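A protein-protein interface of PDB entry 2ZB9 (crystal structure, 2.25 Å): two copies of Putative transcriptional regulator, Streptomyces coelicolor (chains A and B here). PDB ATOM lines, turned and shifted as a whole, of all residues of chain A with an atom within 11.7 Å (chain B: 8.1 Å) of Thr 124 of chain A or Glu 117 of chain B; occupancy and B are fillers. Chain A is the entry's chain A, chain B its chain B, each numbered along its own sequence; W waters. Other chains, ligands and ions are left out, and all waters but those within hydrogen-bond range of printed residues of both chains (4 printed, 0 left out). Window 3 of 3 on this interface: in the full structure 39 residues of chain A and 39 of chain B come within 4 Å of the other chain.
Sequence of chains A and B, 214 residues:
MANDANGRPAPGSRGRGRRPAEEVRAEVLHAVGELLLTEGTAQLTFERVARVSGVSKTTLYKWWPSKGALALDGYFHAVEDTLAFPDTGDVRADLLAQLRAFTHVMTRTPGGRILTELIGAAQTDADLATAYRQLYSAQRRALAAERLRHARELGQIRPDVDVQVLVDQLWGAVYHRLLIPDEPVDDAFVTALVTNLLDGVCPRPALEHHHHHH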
ATOM      1  N   THR A 116      26.041 -14.272   9.371  1.00  0.00           N
ATOM      2  CA  THR A 116      25.402 -15.141   8.377  1.00  0.00           C
ATOM      3  C   THR A 116      24.609 -16.271   9.031  1.00  0.00           C
ATOM      4  O   THR A 116      23.577 -16.700   8.509  1.00  0.00           O
ATOM      5  CB  THR A 116      26.430 -15.770   7.396  1.00  0.00           C
ATOM      6  OG1 THR A 116      27.430 -16.483   8.130  1.00  0.00           O
ATOM      7  CG2 THR A 116      27.096 -14.699   6.554  1.00  0.00           C
ATOM      8  N   GLU A 117      25.082 -16.760  10.170  1.00  0.00           N
ATOM      9  CA  GLU A 117      24.366 -17.828  10.853  1.00  0.00           C
ATOM     10  C   GLU A 117      23.117 -17.295  11.533  1.00  0.00           C
ATOM     11  O   GLU A 117      22.143 -18.025  11.699  1.00  0.00           O
ATOM     12  CB  GLU A 117      25.278 -18.540  11.860  1.00  0.00           C
ATOM     13  CG  GLU A 117      26.362 -19.372  11.174  1.00  0.00           C
ATOM     14  CD  GLU A 117      27.085 -20.321  12.120  1.00  0.00           C
ATOM     15  OE1 GLU A 117      28.005 -21.036  11.658  1.00  0.00           O
ATOM     16  OE2 GLU A 117      26.733 -20.354  13.319  1.00  0.00           O
ATOM     17  N   LEU A 118      23.136 -16.023  11.924  1.00  0.00           N
ATOM     18  CA  LEU A 118      21.957 -15.423  12.546  1.00  0.00           C
ATOM     19  C   LEU A 118      20.919 -15.164  11.446  1.00  0.00           C
ATOM     20  O   LEU A 118      19.715 -15.328  11.655  1.00  0.00           O
ATOM     21  CB  LEU A 118      22.327 -14.110  13.242  1.00  0.00           C
ATOM     22  CG  LEU A 118      23.033 -14.262  14.593  1.00  0.00           C
ATOM     23  CD1 LEU A 118      23.544 -12.907  15.078  1.00  0.00           C
ATOM     24  CD2 LEU A 118      22.052 -14.857  15.598  1.00  0.00           C
ATOM     25  N   ILE A 119      21.395 -14.755  10.273  1.00  0.00           N
ATOM     26  CA  ILE A 119      20.506 -14.513   9.144  1.00  0.00           C
ATOM     27  C   ILE A 119      19.852 -15.850   8.799  1.00  0.00           C
ATOM     28  O   ILE A 119      18.652 -15.926   8.529  1.00  0.00           O
ATOM     29  CB  ILE A 119      21.295 -14.004   7.917  1.00  0.00           C
ATOM     30  CG1 ILE A 119      21.816 -12.587   8.190  1.00  0.00           C
ATOM     31  CG2 ILE A 119      20.406 -14.013   6.667  1.00  0.00           C
ATOM     32  CD1 ILE A 119      22.807 -12.089   7.162  1.00  0.00           C
ATOM     33  N   GLY A 120      20.655 -16.909   8.826  1.00  0.00           N
ATOM     34  CA  GLY A 120      20.140 -18.228   8.517  1.00  0.00           C
ATOM     35  C   GLY A 120      19.068 -18.672   9.489  1.00  0.00           C
ATOM     36  O   GLY A 120      18.000 -19.124   9.081  1.00  0.00           O
ATOM     37  N   ALA A 121      19.349 -18.545  10.781  1.00  0.00           N
ATOM     38  CA  ALA A 121      18.385 -18.943  11.809  1.00  0.00           C
ATOM     39  C   ALA A 121      17.097 -18.120  11.716  1.00  0.00           C
ATOM     40  O   ALA A 121      15.999 -18.634  11.933  1.00  0.00           O
ATOM     41  CB  ALA A 121      19.019 -18.790  13.208  1.00  0.00           C
ATOM     42  N   ALA A 122      17.239 -16.842  11.386  1.00  0.00           N
ATOM     43  CA  ALA A 122      16.096 -15.945  11.267  1.00  0.00           C
ATOM     44  C   ALA A 122      15.074 -16.421  10.246  1.00  0.00           C
ATOM     45  O   ALA A 122      13.890 -16.100  10.354  1.00  0.00           O
ATOM     46  CB  ALA A 122      16.570 -14.548  10.889  1.00  0.00           C
ATOM     47  N   GLN A 123      15.528 -17.185   9.255  1.00  0.00           N
ATOM     48  CA  GLN A 123      14.630 -17.665   8.212  1.00  0.00           C
ATOM     49  C   GLN A 123      13.493 -18.541   8.721  1.00  0.00           C
ATOM     50  O   GLN A 123      12.476 -18.673   8.048  1.00  0.00           O
ATOM     51  CB  GLN A 123      15.418 -18.406   7.125  1.00  0.00           C
ATOM     52  CG  GLN A 123      16.451 -17.528   6.425  1.00  0.00           C
ATOM     53  CD  GLN A 123      15.894 -16.160   6.051  1.00  0.00           C
ATOM     54  OE1 GLN A 123      14.902 -16.056   5.321  1.00  0.00           O
ATOM     55  NE2 GLN A 123      16.531 -15.103   6.553  1.00  0.00           N
ATOM     56  N   THR A 124      13.654 -19.131   9.903  1.00  0.00           N
ATOM     57  CA  THR A 124      12.606 -19.981  10.469  1.00  0.00           C
ATOM     58  C   THR A 124      12.298 -19.641  11.927  1.00  0.00           C
ATOM     59  O   THR A 124      11.800 -20.477  12.677  1.00  0.00           O
ATOM     60  CB  THR A 124      12.980 -21.478  10.399  1.00  0.00           C
ATOM     61  OG1 THR A 124      14.244 -21.687  11.040  1.00  0.00           O
ATOM     62  CG2 THR A 124      13.052 -21.950   8.948  1.00  0.00           C
ATOM     63  N   ASP A 125      12.597 -18.410  12.321  1.00  0.00           N
ATOM     64  CA  ASP A 125      12.353 -17.948  13.686  1.00  0.00           C
ATOM     65  C   ASP A 125      11.898 -16.503  13.559  1.00  0.00           C
ATOM     66  O   ASP A 125      12.716 -15.589  13.487  1.00  0.00           O
ATOM     67  CB  ASP A 125      13.640 -18.025  14.509  1.00  0.00           C
ATOM     68  CG  ASP A 125      13.416 -17.709  15.976  1.00  0.00           C
ATOM     69  OD1 ASP A 125      12.502 -16.914  16.289  1.00  0.00           O
ATOM     70  OD2 ASP A 125      14.166 -18.247  16.820  1.00  0.00           O
ATOM     71  N   ALA A 126      10.584 -16.314  13.520  1.00  0.00           N
ATOM     72  CA  ALA A 126       9.982 -14.997  13.355  1.00  0.00           C
ATOM     73  C   ALA A 126      10.486 -13.947  14.328  1.00  0.00           C
ATOM     74  O   ALA A 126      10.727 -12.807  13.937  1.00  0.00           O
ATOM     75  CB  ALA A 126       8.459 -15.109  13.448  1.00  0.00           C
ATOM     76  N   ASP A 127      10.633 -14.328  15.595  1.00  0.00           N
ATOM     77  CA  ASP A 127      11.107 -13.406  16.618  1.00  0.00           C
ATOM     78  C   ASP A 127      12.556 -12.985  16.388  1.00  0.00           C
ATOM     79  O   ASP A 127      12.906 -11.821  16.575  1.00  0.00           O
ATOM     80  CB  ASP A 127      10.966 -14.032  18.005  1.00  0.00           C
ATOM     81  CG  ASP A 127       9.517 -14.224  18.414  1.00  0.00           C
ATOM     82  OD1 ASP A 127       8.736 -13.251  18.333  1.00  0.00           O
ATOM     83  OD2 ASP A 127       9.158 -15.348  18.828  1.00  0.00           O
ATOM     84  N   LEU A 128      13.401 -13.927  15.986  1.00  0.00           N
ATOM     85  CA  LEU A 128      14.795 -13.599  15.739  1.00  0.00           C
ATOM     86  C   LEU A 128      14.889 -12.657  14.531  1.00  0.00           C
ATOM     87  O   LEU A 128      15.662 -11.693  14.542  1.00  0.00           O
ATOM     88  CB  LEU A 128      15.606 -14.879  15.501  1.00  0.00           C
ATOM     89  CG  LEU A 128      17.116 -14.713  15.305  1.00  0.00           C
ATOM     90  CD1 LEU A 128      17.723 -14.061  16.542  1.00  0.00           C
ATOM     91  CD2 LEU A 128      17.755 -16.071  15.045  1.00  0.00           C
ATOM     92  N   ALA A 129      14.094 -12.929  13.500  1.00  0.00           N
ATOM     93  CA  ALA A 129      14.088 -12.093  12.304  1.00  0.00           C
ATOM     94  C   ALA A 129      13.735 -10.659  12.690  1.00  0.00           C
ATOM     95  O   ALA A 129      14.351  -9.709  12.217  1.00  0.00           O
ATOM     96  CB  ALA A 129      13.078 -12.631  11.278  1.00  0.00           C
ATOM     97  N   THR A 130      12.742 -10.504  13.558  1.00  0.00           N
ATOM     98  CA  THR A 130      12.335  -9.175  14.001  1.00  0.00           C
ATOM     99  C   THR A 130      13.463  -8.470  14.746  1.00  0.00           C
ATOM    100  O   THR A 130      13.702  -7.281  14.540  1.00  0.00           O
ATOM    101  CB  THR A 130      11.092  -9.251  14.912  1.00  0.00           C
ATOM    102  OG1 THR A 130       9.968  -9.684  14.136  1.00  0.00           O
ATOM    103  CG2 THR A 130      10.786  -7.891  15.533  1.00  0.00           C
ATOM    104  N   ALA A 131      14.156  -9.206  15.610  1.00  0.00           N
ATOM    105  CA  ALA A 131      15.266  -8.645  16.378  1.00  0.00           C
ATOM    106  C   ALA A 131      16.446  -8.289  15.465  1.00  0.00           C
ATOM    107  O   ALA A 131      17.153  -7.304  15.696  1.00  0.00           O
ATOM    108  CB  ALA A 131      15.711  -9.636  17.444  1.00  0.00           C
ATOM    109  N   TYR A 132      16.661  -9.095  14.433  1.00  0.00           N
ATOM    110  CA  TYR A 132      17.759  -8.838  13.508  1.00  0.00           C
ATOM    111  C   TYR A 132      17.578  -7.465  12.849  1.00  0.00           C
ATOM    112  O   TYR A 132      18.532  -6.684  12.724  1.00  0.00           O
ATOM    113  CB  TYR A 132      17.808  -9.932  12.439  1.00  0.00           C
ATOM    114  CG  TYR A 132      19.029  -9.849  11.554  1.00  0.00           C
ATOM    115  CD1 TYR A 132      20.204 -10.520  11.888  1.00  0.00           C
ATOM    116  CD2 TYR A 132      19.019  -9.065  10.399  1.00  0.00           C
ATOM    117  CE1 TYR A 132      21.343 -10.415  11.090  1.00  0.00           C
ATOM    118  CE2 TYR A 132      20.152  -8.952   9.596  1.00  0.00           C
ATOM    119  CZ  TYR A 132      21.309  -9.628   9.947  1.00  0.00           C
ATOM    120  OH  TYR A 132      22.428  -9.510   9.157  1.00  0.00           O
ATOM    121  N   ARG A 133      16.350  -7.170  12.437  1.00  0.00           N
ATOM    122  CA  ARG A 133      16.046  -5.885  11.811  1.00  0.00           C
ATOM    123  C   ARG A 133      16.107  -4.730  12.814  1.00  0.00           C
ATOM    124  O   ARG A 133      16.744  -3.704  12.565  1.00  0.00           O
ATOM    125  CB  ARG A 133      14.649  -5.914  11.168  1.00  0.00           C
ATOM    126  CG  ARG A 133      14.520  -6.836   9.952  1.00  0.00           C
ATOM    127  CD  ARG A 133      13.254  -6.527   9.143  1.00  0.00           C
ATOM    128  NE  ARG A 133      12.029  -6.909   9.847  1.00  0.00           N
ATOM    129  CZ  ARG A 133      11.592  -8.162   9.964  1.00  0.00           C
ATOM    130  NH1 ARG A 133      12.276  -9.162   9.420  1.00  0.00           N
ATOM    131  NH2 ARG A 133      10.473  -8.421  10.631  1.00  0.00           N
ATOM    132  N   LEU A 179      26.256 -15.508   1.655  1.00  0.00           N
ATOM    133  CA  LEU A 179      25.282 -16.531   2.058  1.00  0.00           C
ATOM    134  C   LEU A 179      25.352 -17.768   1.160  1.00  0.00           C
ATOM    135  O   LEU A 179      25.141 -18.892   1.615  1.00  0.00           O
ATOM    136  CB  LEU A 179      23.850 -15.974   2.041  1.00  0.00           C
ATOM    137  CG  LEU A 179      23.252 -15.203   3.236  1.00  0.00           C
ATOM    138  CD1 LEU A 179      23.872 -15.681   4.544  1.00  0.00           C
ATOM    139  CD2 LEU A 179      23.455 -13.726   3.066  1.00  0.00           C
ATOM    140  N   ILE A 180      25.628 -17.556  -0.122  1.00  0.00           N
ATOM    141  CA  ILE A 180      25.757 -18.660  -1.063  1.00  0.00           C
ATOM    142  C   ILE A 180      26.970 -18.352  -1.947  1.00  0.00           C
ATOM    143  O   ILE A 180      26.879 -17.687  -2.983  1.00  0.00           O
ATOM    144  CB  ILE A 180      24.434 -18.867  -1.859  1.00  0.00           C
ATOM    145  CG1 ILE A 180      24.728 -19.274  -3.293  1.00  0.00           C
ATOM    146  CG2 ILE A 180      23.545 -17.644  -1.739  1.00  0.00           C
ATOM    147  CD1 ILE A 180      23.491 -19.373  -4.121  1.00  0.00           C
ATOM    148  N   GLY B  40       4.759 -25.898  -0.743  1.00  0.00           N
ATOM    149  CA  GLY B  40       6.056 -25.759  -0.112  1.00  0.00           C
ATOM    150  C   GLY B  40       6.715 -27.081   0.228  1.00  0.00           C
ATOM    151  O   GLY B  40       6.358 -28.125  -0.317  1.00  0.00           O
ATOM    152  N   THR B  41       7.666 -27.036   1.154  1.00  0.00           N
ATOM    153  CA  THR B  41       8.421 -28.217   1.555  1.00  0.00           C
ATOM    154  C   THR B  41       7.984 -28.878   2.856  1.00  0.00           C
ATOM    155  O   THR B  41       8.393 -30.000   3.141  1.00  0.00           O
ATOM    156  CB  THR B  41       9.902 -27.867   1.716  1.00  0.00           C
ATOM    157  OG1 THR B  41      10.026 -26.804   2.670  1.00  0.00           O
ATOM    158  CG2 THR B  41      10.503 -27.422   0.392  1.00  0.00           C
ATOM    159  N   ALA B  42       7.168 -28.187   3.641  1.00  0.00           N
ATOM    160  CA  ALA B  42       6.718 -28.704   4.932  1.00  0.00           C
ATOM    161  C   ALA B  42       6.365 -30.190   4.931  1.00  0.00           C
ATOM    162  O   ALA B  42       6.842 -30.941   5.781  1.00  0.00           O
ATOM    163  CB  ALA B  42       5.534 -27.885   5.437  1.00  0.00           C
ATOM    164  N   LYS B  67      16.241 -34.477   2.024  1.00  0.00           N
ATOM    165  CA  LYS B  67      14.988 -33.838   1.658  1.00  0.00           C
ATOM    166  C   LYS B  67      15.328 -32.558   0.907  1.00  0.00           C
ATOM    167  O   LYS B  67      14.648 -32.188  -0.045  1.00  0.00           O
ATOM    168  CB  LYS B  67      14.179 -33.502   2.915  1.00  0.00           C
ATOM    169  CG  LYS B  67      12.888 -32.748   2.642  1.00  0.00           C
ATOM    170  CD  LYS B  67      12.157 -32.406   3.928  1.00  0.00           C
ATOM    171  CE  LYS B  67      10.941 -31.535   3.658  1.00  0.00           C
ATOM    172  NZ  LYS B  67      10.256 -31.112   4.918  1.00  0.00           N
ATOM    173  N   PRO B 110       5.327 -20.287  -3.715  1.00  0.00           N
ATOM    174  CA  PRO B 110       6.114 -20.683  -2.540  1.00  0.00           C
ATOM    175  C   PRO B 110       7.634 -20.633  -2.763  1.00  0.00           C
ATOM    176  O   PRO B 110       8.420 -20.812  -1.821  1.00  0.00           O
ATOM    177  CB  PRO B 110       5.624 -22.108  -2.258  1.00  0.00           C
ATOM    178  CG  PRO B 110       4.197 -22.101  -2.800  1.00  0.00           C
ATOM    179  CD  PRO B 110       4.391 -21.358  -4.106  1.00  0.00           C
ATOM    180  N   GLY B 111       8.041 -20.397  -4.011  1.00  0.00           N
ATOM    181  CA  GLY B 111       9.456 -20.342  -4.342  1.00  0.00           C
ATOM    182  C   GLY B 111      10.317 -19.522  -3.398  1.00  0.00           C
ATOM    183  O   GLY B 111      11.387 -19.963  -2.988  1.00  0.00           O
ATOM    184  N   GLY B 112       9.868 -18.322  -3.050  1.00  0.00           N
ATOM    185  CA  GLY B 112      10.646 -17.489  -2.143  1.00  0.00           C
ATOM    186  C   GLY B 112      10.857 -18.094  -0.762  1.00  0.00           C
ATOM    187  O   GLY B 112      11.973 -18.083  -0.223  1.00  0.00           O
ATOM    188  N   ARG B 113       9.787 -18.619  -0.176  1.00  0.00           N
ATOM    189  CA  ARG B 113       9.867 -19.236   1.144  1.00  0.00           C
ATOM    190  C   ARG B 113      10.723 -20.491   1.063  1.00  0.00           C
ATOM    191  O   ARG B 113      11.509 -20.792   1.963  1.00  0.00           O
ATOM    192  CB  ARG B 113       8.460 -19.576   1.646  1.00  0.00           C
ATOM    193  CG  ARG B 113       7.836 -18.514   2.556  1.00  0.00           C
ATOM    194  CD  ARG B 113       8.106 -17.085   2.081  1.00  0.00           C
ATOM    195  NE  ARG B 113       7.266 -16.664   0.959  1.00  0.00           N
ATOM    196  CZ  ARG B 113       7.458 -15.544   0.267  1.00  0.00           C
ATOM    197  NH1 ARG B 113       8.462 -14.733   0.578  1.00  0.00           N
ATOM    198  NH2 ARG B 113       6.648 -15.233  -0.738  1.00  0.00           N
ATOM    199  N   ILE B 114      10.583 -21.218  -0.037  1.00  0.00           N
ATOM    200  CA  ILE B 114      11.357 -22.433  -0.230  1.00  0.00           C
ATOM    201  C   ILE B 114      12.859 -22.143  -0.244  1.00  0.00           C
ATOM    202  O   ILE B 114      13.618 -22.749   0.509  1.00  0.00           O
ATOM    203  CB  ILE B 114      10.960 -23.141  -1.554  1.00  0.00           C
ATOM    204  CG1 ILE B 114       9.518 -23.657  -1.443  1.00  0.00           C
ATOM    205  CG2 ILE B 114      11.926 -24.272  -1.853  1.00  0.00           C
ATOM    206  CD1 ILE B 114       8.927 -24.193  -2.744  1.00  0.00           C
ATOM    207  N   LEU B 115      13.291 -21.210  -1.085  1.00  0.00           N
ATOM    208  CA  LEU B 115      14.712 -20.916  -1.166  1.00  0.00           C
ATOM    209  C   LEU B 115      15.294 -20.250   0.068  1.00  0.00           C
ATOM    210  O   LEU B 115      16.404 -20.587   0.471  1.00  0.00           O
ATOM    211  CB  LEU B 115      15.020 -20.071  -2.405  1.00  0.00           C
ATOM    212  CG  LEU B 115      14.782 -20.779  -3.746  1.00  0.00           C
ATOM    213  CD1 LEU B 115      15.232 -19.860  -4.872  1.00  0.00           C
ATOM    214  CD2 LEU B 115      15.544 -22.108  -3.792  1.00  0.00           C
ATOM    215  N   THR B 116      14.569 -19.313   0.678  1.00  0.00           N
ATOM    216  CA  THR B 116      15.107 -18.655   1.870  1.00  0.00           C
ATOM    217  C   THR B 116      15.296 -19.644   3.015  1.00  0.00           C
ATOM    218  O   THR B 116      16.278 -19.557   3.750  1.00  0.00           O
ATOM    219  CB  THR B 116      14.215 -17.497   2.369  1.00  0.00           C
ATOM    220  OG1 THR B 116      12.873 -17.959   2.539  1.00  0.00           O
ATOM    221  CG2 THR B 116      14.245 -16.338   1.392  1.00  0.00           C
ATOM    222  N   GLU B 117      14.367 -20.585   3.167  1.00  0.00           N
ATOM    223  CA  GLU B 117      14.483 -21.579   4.229  1.00  0.00           C
ATOM    224  C   GLU B 117      15.719 -22.422   3.950  1.00  0.00           C
ATOM    225  O   GLU B 117      16.566 -22.599   4.820  1.00  0.00           O
ATOM    226  CB  GLU B 117      13.253 -22.490   4.282  1.00  0.00           C
ATOM    227  CG  GLU B 117      13.270 -23.430   5.491  1.00  0.00           C
ATOM    228  CD  GLU B 117      12.278 -24.579   5.389  1.00  0.00           C
ATOM    229  OE1 GLU B 117      11.120 -24.340   4.984  1.00  0.00           O
ATOM    230  OE2 GLU B 117      12.658 -25.722   5.730  1.00  0.00           O
ATOM    231  N   LEU B 118      15.822 -22.933   2.725  1.00  0.00           N
ATOM    232  CA  LEU B 118      16.971 -23.744   2.330  1.00  0.00           C
ATOM    233  C   LEU B 118      18.273 -22.966   2.506  1.00  0.00           C
ATOM    234  O   LEU B 118      19.255 -23.494   3.028  1.00  0.00           O
ATOM    235  CB  LEU B 118      16.839 -24.197   0.870  1.00  0.00           C
ATOM    236  CG  LEU B 118      15.994 -25.440   0.545  1.00  0.00           C
ATOM    237  CD1 LEU B 118      16.628 -26.674   1.162  1.00  0.00           C
ATOM    238  CD2 LEU B 118      14.587 -25.266   1.080  1.00  0.00           C
ATOM    239  N   ILE B 119      18.289 -21.711   2.064  1.00  0.00           N
ATOM    240  CA  ILE B 119      19.493 -20.900   2.195  1.00  0.00           C
ATOM    241  C   ILE B 119      19.813 -20.771   3.680  1.00  0.00           C
ATOM    242  O   ILE B 119      20.971 -20.879   4.091  1.00  0.00           O
ATOM    243  CB  ILE B 119      19.304 -19.484   1.589  1.00  0.00           C
ATOM    244  CG1 ILE B 119      19.184 -19.573   0.066  1.00  0.00           C
ATOM    245  CG2 ILE B 119      20.491 -18.600   1.939  1.00  0.00           C
ATOM    246  CD1 ILE B 119      18.756 -18.266  -0.582  1.00  0.00           C
ATOM    247  N   GLY B 120      18.773 -20.546   4.479  1.00  0.00           N
ATOM    248  CA  GLY B 120      18.966 -20.410   5.910  1.00  0.00           C
ATOM    249  C   GLY B 120      19.616 -21.636   6.522  1.00  0.00           C
ATOM    250  O   GLY B 120      20.610 -21.528   7.230  1.00  0.00           O
ATOM    251  N   ALA B 121      19.052 -22.804   6.237  1.00  0.00           N
ATOM    252  CA  ALA B 121      19.551 -24.070   6.765  1.00  0.00           C
ATOM    253  C   ALA B 121      20.963 -24.376   6.306  1.00  0.00           C
ATOM    254  O   ALA B 121      21.751 -24.953   7.056  1.00  0.00           O
ATOM    255  CB  ALA B 121      18.615 -25.212   6.356  1.00  0.00           C
ATOM    256  N   ALA B 122      21.287 -23.985   5.078  1.00  0.00           N
ATOM    257  CA  ALA B 122      22.614 -24.241   4.525  1.00  0.00           C
ATOM    258  C   ALA B 122      23.736 -23.576   5.315  1.00  0.00           C
ATOM    259  O   ALA B 122      24.884 -24.024   5.264  1.00  0.00           O
ATOM    260  CB  ALA B 122      22.670 -23.780   3.073  1.00  0.00           C
ATOM    261  N   GLN B 123      23.411 -22.511   6.041  1.00  0.00           N
ATOM    262  CA  GLN B 123      24.418 -21.795   6.813  1.00  0.00           C
ATOM    263  C   GLN B 123      25.079 -22.653   7.890  1.00  0.00           C
ATOM    264  O   GLN B 123      26.173 -22.336   8.354  1.00  0.00           O
ATOM    265  CB  GLN B 123      23.807 -20.537   7.440  1.00  0.00           C
ATOM    266  CG  GLN B 123      23.213 -19.576   6.418  1.00  0.00           C
ATOM    267  CD  GLN B 123      24.136 -19.360   5.226  1.00  0.00           C
ATOM    268  OE1 GLN B 123      25.306 -18.987   5.383  1.00  0.00           O
ATOM    269  NE2 GLN B 123      23.615 -19.597   4.026  1.00  0.00           N
ATOM    270  N   LEU B 128      24.155 -29.550   2.542  1.00  0.00           N
ATOM    271  CA  LEU B 128      23.011 -28.868   1.952  1.00  0.00           C
ATOM    272  C   LEU B 128      23.488 -27.649   1.172  1.00  0.00           C
ATOM    273  O   LEU B 128      22.935 -27.316   0.129  1.00  0.00           O
ATOM    274  CB  LEU B 128      22.021 -28.441   3.036  1.00  0.00           C
ATOM    275  CG  LEU B 128      20.774 -27.683   2.566  1.00  0.00           C
ATOM    276  CD1 LEU B 128      19.959 -28.547   1.611  1.00  0.00           C
ATOM    277  CD2 LEU B 128      19.935 -27.294   3.777  1.00  0.00           C
ATOM    278  N   TYR B 132      22.815 -27.046  -2.660  1.00  0.00           N
ATOM    279  CA  TYR B 132      22.135 -25.833  -3.101  1.00  0.00           C
ATOM    280  C   TYR B 132      22.819 -25.257  -4.330  1.00  0.00           C
ATOM    281  O   TYR B 132      22.162 -24.832  -5.283  1.00  0.00           O
ATOM    282  CB  TYR B 132      22.119 -24.796  -1.969  1.00  0.00           C
ATOM    283  CG  TYR B 132      21.275 -23.569  -2.252  1.00  0.00           C
ATOM    284  CD1 TYR B 132      21.727 -22.564  -3.103  1.00  0.00           C
ATOM    285  CD2 TYR B 132      20.019 -23.420  -1.671  1.00  0.00           C
ATOM    286  CE1 TYR B 132      20.947 -21.442  -3.368  1.00  0.00           C
ATOM    287  CE2 TYR B 132      19.234 -22.307  -1.931  1.00  0.00           C
ATOM    288  CZ  TYR B 132      19.702 -21.319  -2.781  1.00  0.00           C
ATOM    289  OH  TYR B 132      18.918 -20.216  -3.040  1.00  0.00           O
ATOM    290  N   LEU B 179      15.617 -12.211   2.078  1.00  0.00           N
ATOM    291  CA  LEU B 179      16.224 -12.786   3.279  1.00  0.00           C
ATOM    292  C   LEU B 179      16.151 -11.852   4.496  1.00  0.00           C
ATOM    293  O   LEU B 179      16.008 -12.316   5.624  1.00  0.00           O
ATOM    294  CB  LEU B 179      17.693 -13.134   3.018  1.00  0.00           C
ATOM    295  CG  LEU B 179      18.045 -14.408   2.242  1.00  0.00           C
ATOM    296  CD1 LEU B 179      17.654 -15.644   3.046  1.00  0.00           C
ATOM    297  CD2 LEU B 179      17.329 -14.405   0.912  1.00  0.00           C
HETATM  298  O   HOH W   1      26.902 -19.008   7.750  1.00  0.00           O
HETATM  299  O   HOH W   2      13.204 -14.035   5.035  1.00  0.00           O
HETATM  300  O   HOH W   3      27.443 -19.139   4.036  1.00  0.00           O
HETATM  301  O   HOH W   4      28.529 -20.779   8.672  1.00  0.00           O
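The side-chain amide nitrogen (NE2) of Gln 123 of chain A lies within hydrogen-bond range of the backbone carbonyl oxygen (O) of Leu 179 of chain B. The backbone carbonyl oxygen (O) of Leu 179 of chain A is in hydrogen-bond range of the side-chain amide nitrogen (NE2) of Gln 123 of chain B (2.9 Å).
Of the printed residues of chain B, Thr 116 of chain A touches Gln 123. Printed residues of chain B within 4 Å of Gln 123 of chain A: Thr 116, Gly 120 and Leu 179. Of chain B, only Glu 117 comes within 4 Å of Thr 124 of chain A. Tyr 132 of chain A touches none of the printed residues of chain B. Printed residues of chain B within 4 Å of Leu 179 of chain A: Gln 123. Thr 116 of chain B touches just one residue of chain A: Gln 123 (3.4 Å). Of chain A, only Thr 124 comes within 4 Å of Glu 117 of chain B. No residue of chain A comes within 4 Å of Leu 118 of chain B. No residue of chain A comes within 4 Å of Ile 119 of chain B. Printed residues of chain A within 4 Å of Tyr 132 of chain B: Ile 180.
Among the printed residues, pairs that only touch across the chains: Gln 123 of chain A with Thr 116 of chain B (3.4 Å), Ile 180 of chain A with Tyr 132 of chain B (3.4 Å), Gly 120 of chain A with Gly 120 of chain B (3.6 Å), Thr 116 of chain A with Gln 123 of chain B (3.6 Å), Thr 124 of chain A with Glu 117 of chain B (3.8 Å), Gln 123 of chain A with Gly 120 of chain B (3.9 Å), Gly 120 of chain A with Gln 123 of chain B (3.96 Å) and Glu 117 of chain A with Gln 123 of chain B (3.995 Å).
Glu 117 of chain A touches Gln 123 of chain B, but with the chains exchanged Gln 123 of chain A does not touch Glu 117 of chain B (4.4 Å). Gly 120 of chain A touches its own counterpart, Gly 120 of chain B. Positions printed for both chains: 116, 117, 118, 119, 120, 121, 122, 123, 128, 132 and 179. Of the 10 pairs that touch across the chains among the printed residues, 7 have their exchanged pair printed and touching as well.
Water W3 bridges the side-chain amide oxygen (OE1) of Gln 123 of chain B and the backbone carbonyl oxygen (O) of Leu 179 of chain A. Water W1 lies within hydrogen-bond range of the side-chain hydroxyl (OG1) of Thr 116 of chain A and the side-chain amide oxygen (OE1) of Gln 123 of chain B. Water W2 bridges OE1 of Gln 123 of chain A and O of Leu 179 of chain B. Water W4 bridges O of Gln 123 of chain B and OE1 of Glu 117 of chain A.
The backbone carbonyl oxygen (O) of Gly 112 of chain B sits at hydrogen-bond distance from the side-chain hydroxyl (OG1) of Thr 116 of chain B (2.9 Å). The backbone carbonyl oxygen of Arg 113 of chain B lies within hydrogen-bond range of the side-chain hydroxyl of Thr 116 of chain B, at 3.2 Å.
Printed residues of chain B that touch a printed residue of chain A: Thr 116, Glu 117, Gly 120, Gln 123, Tyr 132 and Leu 179. Hydrophobic or aromatic side chains of chain B that line the printed part of chain A: Tyr 132 and Leu 179. Of the 20 printed residues of chain A, 7 touch a printed residue of chain B. Hydrophobic or aromatic side chains of chain A that line the printed part of chain B: Leu 179 and Ile 180. Among the printed residues, 10 pairs touch across the chains.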
